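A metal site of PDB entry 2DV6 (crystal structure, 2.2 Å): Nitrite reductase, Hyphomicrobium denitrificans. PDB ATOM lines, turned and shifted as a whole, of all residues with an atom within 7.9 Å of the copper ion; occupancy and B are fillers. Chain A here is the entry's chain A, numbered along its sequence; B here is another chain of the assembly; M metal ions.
ND1 of His 119 sits close to O of Gln 76.
The backbone carbonyl oxygen (O) of Met 40 is in hydrogen-bond range of the backbone NH (N) of Met 124, 3.3 Å away.
The backbone NH (N) of Cys 114 sits at hydrogen-bond distance from the side-chain hydroxyl (OH) of Tyr 42 (3.0 Å).
The side-chain hydroxyl of Thr 33 lies close to a ring nitrogen (NE2) of His 77, at 3.4 Å.
O of Met 124 lies within hydrogen-bond range of N of Cys 114 (3.1 Å).
The backbone carbonyl oxygen (O) of His 119 is in hydrogen-bond range of the backbone NH (N) of Met 124, at 2.9 Å.
NE2 of His 77 sits close to O of Ala 75.
ND1 of His 77 sits close to SD of Met 124 (3.3 Å).
Gln 76 touches the copper ion (O to CU, 3.3 Å).
Of the 24 residues printed, 5 come within 4 Å of the copper ion.
The copper ion is bound by ND1 of His 119 (2.1 Å), ND1 of His 77 (2.1 Å) and SG of Cys 114 (2.2 Å).
Slightly farther from the copper ion lies the side-chain sulfur (SD) of Met 124 (2.9 Å).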
ATOM      1  N   THR A  33      14.997   0.795  26.631  1.00  0.00           N
ATOM      2  CA  THR A  33      16.271   0.954  25.938  1.00  0.00           C
ATOM      3  C   THR A  33      16.327   2.390  25.351  1.00  0.00           C
ATOM      4  O   THR A  33      15.287   2.986  25.042  1.00  0.00           O
ATOM      5  CB  THR A  33      16.464  -0.114  24.831  1.00  0.00           C
ATOM      6  OG1 THR A  33      15.544   0.140  23.761  1.00  0.00           O
ATOM      7  CG2 THR A  33      16.242  -1.554  25.374  1.00  0.00           C
ATOM      8  N   MET A  40      24.350   3.744  23.731  1.00  0.00           N
ATOM      9  CA  MET A  40      23.147   2.905  23.734  1.00  0.00           C
ATOM     10  C   MET A  40      23.126   2.151  25.046  1.00  0.00           C
ATOM     11  O   MET A  40      24.081   1.444  25.362  1.00  0.00           O
ATOM     12  CB  MET A  40      23.197   1.928  22.570  1.00  0.00           C
ATOM     13  CG  MET A  40      21.863   1.217  22.277  1.00  0.00           C
ATOM     14  SD  MET A  40      22.053   0.170  20.801  1.00  0.00           S
ATOM     15  CE  MET A  40      21.191   1.248  19.691  1.00  0.00           C
ATOM     16  N   VAL A  41      22.057   2.320  25.808  1.00  0.00           N
ATOM     17  CA  VAL A  41      22.014   1.891  27.201  1.00  0.00           C
ATOM     18  C   VAL A  41      20.612   1.416  27.581  1.00  0.00           C
ATOM     19  O   VAL A  41      19.702   1.490  26.756  1.00  0.00           O
ATOM     20  CB  VAL A  41      22.389   3.046  28.156  1.00  0.00           C
ATOM     21  CG1 VAL A  41      23.814   3.561  27.840  1.00  0.00           C
ATOM     22  CG2 VAL A  41      21.336   4.185  28.080  1.00  0.00           C
ATOM     23  N   TYR A  42      20.463   0.891  28.794  1.00  0.00           N
ATOM     24  CA  TYR A  42      19.146   0.699  29.395  1.00  0.00           C
ATOM     25  C   TYR A  42      18.890   1.874  30.322  1.00  0.00           C
ATOM     26  O   TYR A  42      19.847   2.402  30.921  1.00  0.00           O
ATOM     27  CB  TYR A  42      19.112  -0.545  30.282  1.00  0.00           C
ATOM     28  CG  TYR A  42      19.372  -1.863  29.595  1.00  0.00           C
ATOM     29  CD1 TYR A  42      20.654  -2.419  29.606  1.00  0.00           C
ATOM     30  CD2 TYR A  42      18.351  -2.549  28.915  1.00  0.00           C
ATOM     31  CE1 TYR A  42      20.920  -3.663  28.979  1.00  0.00           C
ATOM     32  CE2 TYR A  42      18.610  -3.802  28.266  1.00  0.00           C
ATOM     33  CZ  TYR A  42      19.909  -4.347  28.328  1.00  0.00           C
ATOM     34  OH  TYR A  42      20.201  -5.572  27.726  1.00  0.00           O
ATOM     35  N   LEU A  69      11.281  -5.438  29.929  1.00  0.00           N
ATOM     36  CA  LEU A  69      12.109  -4.728  28.971  1.00  0.00           C
ATOM     37  C   LEU A  69      11.190  -4.109  27.941  1.00  0.00           C
ATOM     38  O   LEU A  69      10.390  -4.823  27.324  1.00  0.00           O
ATOM     39  CB  LEU A  69      13.032  -5.731  28.290  1.00  0.00           C
ATOM     40  CG  LEU A  69      14.261  -5.339  27.452  1.00  0.00           C
ATOM     41  CD1 LEU A  69      14.278  -5.975  26.059  1.00  0.00           C
ATOM     42  CD2 LEU A  69      14.704  -3.869  27.488  1.00  0.00           C
ATOM     43  N   ASN A  71      11.351  -1.636  24.462  1.00  0.00           N
ATOM     44  CA  ASN A  71      12.195  -1.101  23.433  1.00  0.00           C
ATOM     45  C   ASN A  71      11.845   0.387  23.263  1.00  0.00           C
ATOM     46  O   ASN A  71      10.670   0.750  23.003  1.00  0.00           O
ATOM     47  CB  ASN A  71      11.965  -1.921  22.141  1.00  0.00           C
ATOM     48  CG  ASN A  71      12.860  -1.514  21.015  1.00  0.00           C
ATOM     49  OD1 ASN A  71      13.096  -0.326  20.790  1.00  0.00           O
ATOM     50  ND2 ASN A  71      13.334  -2.506  20.239  1.00  0.00           N
ATOM     51  N   GLU A  73      13.906   2.807  21.307  1.00  0.00           N
ATOM     52  CA  GLU A  73      14.285   3.535  20.096  1.00  0.00           C
ATOM     53  C   GLU A  73      14.162   2.748  18.794  1.00  0.00           C
ATOM     54  O   GLU A  73      14.267   3.350  17.743  1.00  0.00           O
ATOM     55  CB  GLU A  73      15.689   4.147  20.270  1.00  0.00           C
ATOM     56  CG  GLU A  73      16.852   3.183  20.003  1.00  0.00           C
ATOM     57  CD  GLU A  73      16.796   1.922  20.834  1.00  0.00           C
ATOM     58  OE1 GLU A  73      16.744   2.001  22.075  1.00  0.00           O
ATOM     59  OE2 GLU A  73      16.771   0.844  20.230  1.00  0.00           O
ATOM     60  N   ALA A  75      15.859  -0.359  17.852  1.00  0.00           N
ATOM     61  CA  ALA A  75      16.909  -1.297  17.476  1.00  0.00           C
ATOM     62  C   ALA A  75      16.537  -2.620  18.128  1.00  0.00           C
ATOM     63  O   ALA A  75      15.671  -2.648  19.023  1.00  0.00           O
ATOM     64  CB  ALA A  75      18.264  -0.828  17.956  1.00  0.00           C
ATOM     65  N   GLN A  76      17.145  -3.712  17.691  1.00  0.00           N
ATOM     66  CA  GLN A  76      16.798  -5.006  18.228  1.00  0.00           C
ATOM     67  C   GLN A  76      17.466  -5.175  19.579  1.00  0.00           C
ATOM     68  O   GLN A  76      18.631  -4.792  19.713  1.00  0.00           O
ATOM     69  CB  GLN A  76      17.287  -6.060  17.244  1.00  0.00           C
ATOM     70  CG  GLN A  76      16.795  -7.428  17.488  1.00  0.00           C
ATOM     71  CD  GLN A  76      17.145  -8.342  16.330  1.00  0.00           C
ATOM     72  OE1 GLN A  76      18.265  -8.293  15.793  1.00  0.00           O
ATOM     73  NE2 GLN A  76      16.175  -9.171  15.917  1.00  0.00           N
ATOM     74  N   HIS A  77      16.755  -5.716  20.579  1.00  0.00           N
ATOM     75  CA  HIS A  77      17.338  -5.873  21.933  1.00  0.00           C
ATOM     76  C   HIS A  77      16.873  -7.100  22.694  1.00  0.00           C
ATOM     77  O   HIS A  77      15.803  -7.610  22.449  1.00  0.00           O
ATOM     78  CB  HIS A  77      17.030  -4.671  22.865  1.00  0.00           C
ATOM     79  CG  HIS A  77      17.445  -3.336  22.314  1.00  0.00           C
ATOM     80  ND1 HIS A  77      18.759  -2.995  22.084  1.00  0.00           N
ATOM     81  CD2 HIS A  77      16.711  -2.262  21.950  1.00  0.00           C
ATOM     82  CE1 HIS A  77      18.822  -1.771  21.618  1.00  0.00           C
ATOM     83  NE2 HIS A  77      17.588  -1.305  21.523  1.00  0.00           N
ATOM     84  N   ASP A  78      17.681  -7.532  23.665  1.00  0.00           N
ATOM     85  CA  ASP A  78      17.172  -8.358  24.749  1.00  0.00           C
ATOM     86  C   ASP A  78      17.861  -7.938  26.052  1.00  0.00           C
ATOM     87  O   ASP A  78      18.552  -6.908  26.080  1.00  0.00           O
ATOM     88  CB  ASP A  78      17.275  -9.876  24.458  1.00  0.00           C
ATOM     89  CG  ASP A  78      18.713 -10.374  24.256  1.00  0.00           C
ATOM     90  OD1 ASP A  78      18.867 -11.559  23.813  1.00  0.00           O
ATOM     91  OD2 ASP A  78      19.695  -9.645  24.558  1.00  0.00           O
ATOM     92  N   VAL A  79      17.634  -8.724  27.111  1.00  0.00           N
ATOM     93  CA  VAL A  79      18.395  -8.668  28.346  1.00  0.00           C
ATOM     94  C   VAL A  79      18.756 -10.113  28.679  1.00  0.00           C
ATOM     95  O   VAL A  79      17.890 -10.986  28.692  1.00  0.00           O
ATOM     96  CB  VAL A  79      17.564  -8.212  29.560  1.00  0.00           C
ATOM     97  CG1 VAL A  79      18.495  -7.986  30.771  1.00  0.00           C
ATOM     98  CG2 VAL A  79      16.801  -6.985  29.295  1.00  0.00           C
ATOM     99  N   VAL A  91      13.255  -8.160  21.290  1.00  0.00           N
ATOM    100  CA  VAL A  91      12.279  -7.133  21.125  1.00  0.00           C
ATOM    101  C   VAL A  91      12.745  -6.266  19.950  1.00  0.00           C
ATOM    102  O   VAL A  91      13.844  -5.755  19.943  1.00  0.00           O
ATOM    103  CB  VAL A  91      12.225  -6.514  22.545  1.00  0.00           C
ATOM    104  CG1 VAL A  91      13.046  -5.236  22.785  1.00  0.00           C
ATOM    105  CG2 VAL A  91      10.908  -6.672  23.183  1.00  0.00           C
ATOM    106  N   TYR A 113      22.937  -7.834  30.304  1.00  0.00           N
ATOM    107  CA  TYR A 113      23.478  -7.179  29.100  1.00  0.00           C
ATOM    108  C   TYR A 113      22.621  -7.553  27.899  1.00  0.00           C
ATOM    109  O   TYR A 113      21.816  -8.493  27.953  1.00  0.00           O
ATOM    110  CB  TYR A 113      24.949  -7.594  28.868  1.00  0.00           C
ATOM    111  CG  TYR A 113      25.085  -9.084  28.623  1.00  0.00           C
ATOM    112  CD1 TYR A 113      24.985  -9.620  27.323  1.00  0.00           C
ATOM    113  CD2 TYR A 113      25.279  -9.969  29.679  1.00  0.00           C
ATOM    114  CE1 TYR A 113      25.064 -11.012  27.098  1.00  0.00           C
ATOM    115  CE2 TYR A 113      25.381 -11.358  29.464  1.00  0.00           C
ATOM    116  CZ  TYR A 113      25.256 -11.856  28.183  1.00  0.00           C
ATOM    117  OH  TYR A 113      25.353 -13.196  27.991  1.00  0.00           O
ATOM    118  N   CYS A 114      22.797  -6.804  26.807  1.00  0.00           N
ATOM    119  CA  CYS A 114      22.105  -7.097  25.564  1.00  0.00           C
ATOM    120  C   CYS A 114      22.996  -7.972  24.699  1.00  0.00           C
ATOM    121  O   CYS A 114      24.183  -7.679  24.546  1.00  0.00           O
ATOM    122  CB  CYS A 114      21.713  -5.820  24.823  1.00  0.00           C
ATOM    123  SG  CYS A 114      20.871  -6.192  23.301  1.00  0.00           S
ATOM    124  N   SER A 115      22.414  -9.041  24.116  1.00  0.00           N
ATOM    125  CA  SER A 115      23.188 -10.049  23.414  1.00  0.00           C
ATOM    126  C   SER A 115      23.205  -9.790  21.911  1.00  0.00           C
ATOM    127  O   SER A 115      23.830 -10.525  21.181  1.00  0.00           O
ATOM    128  CB  SER A 115      22.592 -11.446  23.639  1.00  0.00           C
ATOM    129  OG  SER A 115      21.363 -11.557  22.942  1.00  0.00           O
ATOM    130  N   ILE A 116      22.472  -8.774  21.455  1.00  0.00           N
ATOM    131  CA  ILE A 116      22.527  -8.364  20.052  1.00  0.00           C
ATOM    132  C   ILE A 116      23.960  -7.886  19.693  1.00  0.00           C
ATOM    133  O   ILE A 116      24.631  -7.182  20.488  1.00  0.00           O
ATOM    134  CB  ILE A 116      21.420  -7.310  19.756  1.00  0.00           C
ATOM    135  CG1 ILE A 116      20.037  -7.868  20.146  1.00  0.00           C
ATOM    136  CG2 ILE A 116      21.463  -6.823  18.303  1.00  0.00           C
ATOM    137  CD1 ILE A 116      19.724  -9.310  19.604  1.00  0.00           C
ATOM    138  N   ALA A 117      24.446  -8.315  18.511  1.00  0.00           N
ATOM    139  CA  ALA A 117      25.830  -8.034  18.129  1.00  0.00           C
ATOM    140  C   ALA A 117      26.181  -6.539  18.289  1.00  0.00           C
ATOM    141  O   ALA A 117      25.521  -5.662  17.701  1.00  0.00           O
ATOM    142  CB  ALA A 117      26.108  -8.500  16.659  1.00  0.00           C
ATOM    143  N   GLY A 118      27.203  -6.267  19.103  1.00  0.00           N
ATOM    144  CA  GLY A 118      27.721  -4.913  19.273  1.00  0.00           C
ATOM    145  C   GLY A 118      27.118  -4.164  20.449  1.00  0.00           C
ATOM    146  O   GLY A 118      27.754  -3.267  20.992  1.00  0.00           O
ATOM    147  N   HIS A 119      25.911  -4.532  20.863  1.00  0.00           N
ATOM    148  CA  HIS A 119      25.165  -3.731  21.864  1.00  0.00           C
ATOM    149  C   HIS A 119      25.795  -3.712  23.234  1.00  0.00           C
ATOM    150  O   HIS A 119      25.794  -2.659  23.884  1.00  0.00           O
ATOM    151  CB  HIS A 119      23.688  -4.142  21.948  1.00  0.00           C
ATOM    152  CG  HIS A 119      22.937  -3.836  20.700  1.00  0.00           C
ATOM    153  ND1 HIS A 119      21.571  -3.650  20.677  1.00  0.00           N
ATOM    154  CD2 HIS A 119      23.361  -3.686  19.416  1.00  0.00           C
ATOM    155  CE1 HIS A 119      21.186  -3.377  19.442  1.00  0.00           C
ATOM    156  NE2 HIS A 119      22.249  -3.407  18.662  1.00  0.00           N
ATOM    157  N   ARG A 120      26.320  -4.846  23.710  1.00  0.00           N
ATOM    158  CA  ARG A 120      26.983  -4.806  25.029  1.00  0.00           C
ATOM    159  C   ARG A 120      28.205  -3.878  24.961  1.00  0.00           C
ATOM    160  O   ARG A 120      28.409  -3.064  25.864  1.00  0.00           O
ATOM    161  CB  ARG A 120      27.267  -6.188  25.625  1.00  0.00           C
ATOM    162  CG  ARG A 120      28.403  -6.142  26.639  1.00  0.00           C
ATOM    163  CD  ARG A 120      28.237  -6.905  27.954  1.00  0.00           C
ATOM    164  NE  ARG A 120      28.443  -8.322  27.819  1.00  0.00           N
ATOM    165  CZ  ARG A 120      28.663  -9.183  28.829  1.00  0.00           C
ATOM    166  NH1 ARG A 120      28.760  -8.817  30.117  1.00  0.00           N
ATOM    167  NH2 ARG A 120      28.778 -10.451  28.510  1.00  0.00           N
ATOM    168  N   ALA A 122      28.575  -1.341  22.844  1.00  0.00           N
ATOM    169  CA  ALA A 122      27.985  -0.026  22.663  1.00  0.00           C
ATOM    170  C   ALA A 122      27.502   0.615  23.992  1.00  0.00           C
ATOM    171  O   ALA A 122      27.301   1.813  24.044  1.00  0.00           O
ATOM    172  CB  ALA A 122      26.839  -0.113  21.655  1.00  0.00           C
ATOM    173  N   MET A 124      25.255  -1.414  26.484  1.00  0.00           N
ATOM    174  CA  MET A 124      24.105  -2.070  27.084  1.00  0.00           C
ATOM    175  C   MET A 124      24.491  -3.166  28.110  1.00  0.00           C
ATOM    176  O   MET A 124      24.483  -4.357  27.817  1.00  0.00           O
ATOM    177  CB  MET A 124      23.183  -2.599  25.971  1.00  0.00           C
ATOM    178  CG  MET A 124      22.610  -1.486  25.069  1.00  0.00           C
ATOM    179  SD  MET A 124      21.238  -2.071  24.109  1.00  0.00           S
ATOM    180  CE  MET A 124      19.969  -1.942  25.394  1.00  0.00           C
ATOM    181  N   ALA B 122      26.702  -3.480  15.303  1.00  0.00           N
ATOM    182  CA  ALA B 122      25.302  -3.061  15.421  1.00  0.00           C
ATOM    183  C   ALA B 122      24.680  -2.664  14.095  1.00  0.00           C
ATOM    184  O   ALA B 122      23.483  -2.603  13.992  1.00  0.00           O
ATOM    185  CB  ALA B 122      25.141  -1.941  16.478  1.00  0.00           C
HETATM  186 CU    CU M   1      20.460  -4.234  22.367  1.00  0.00          CU
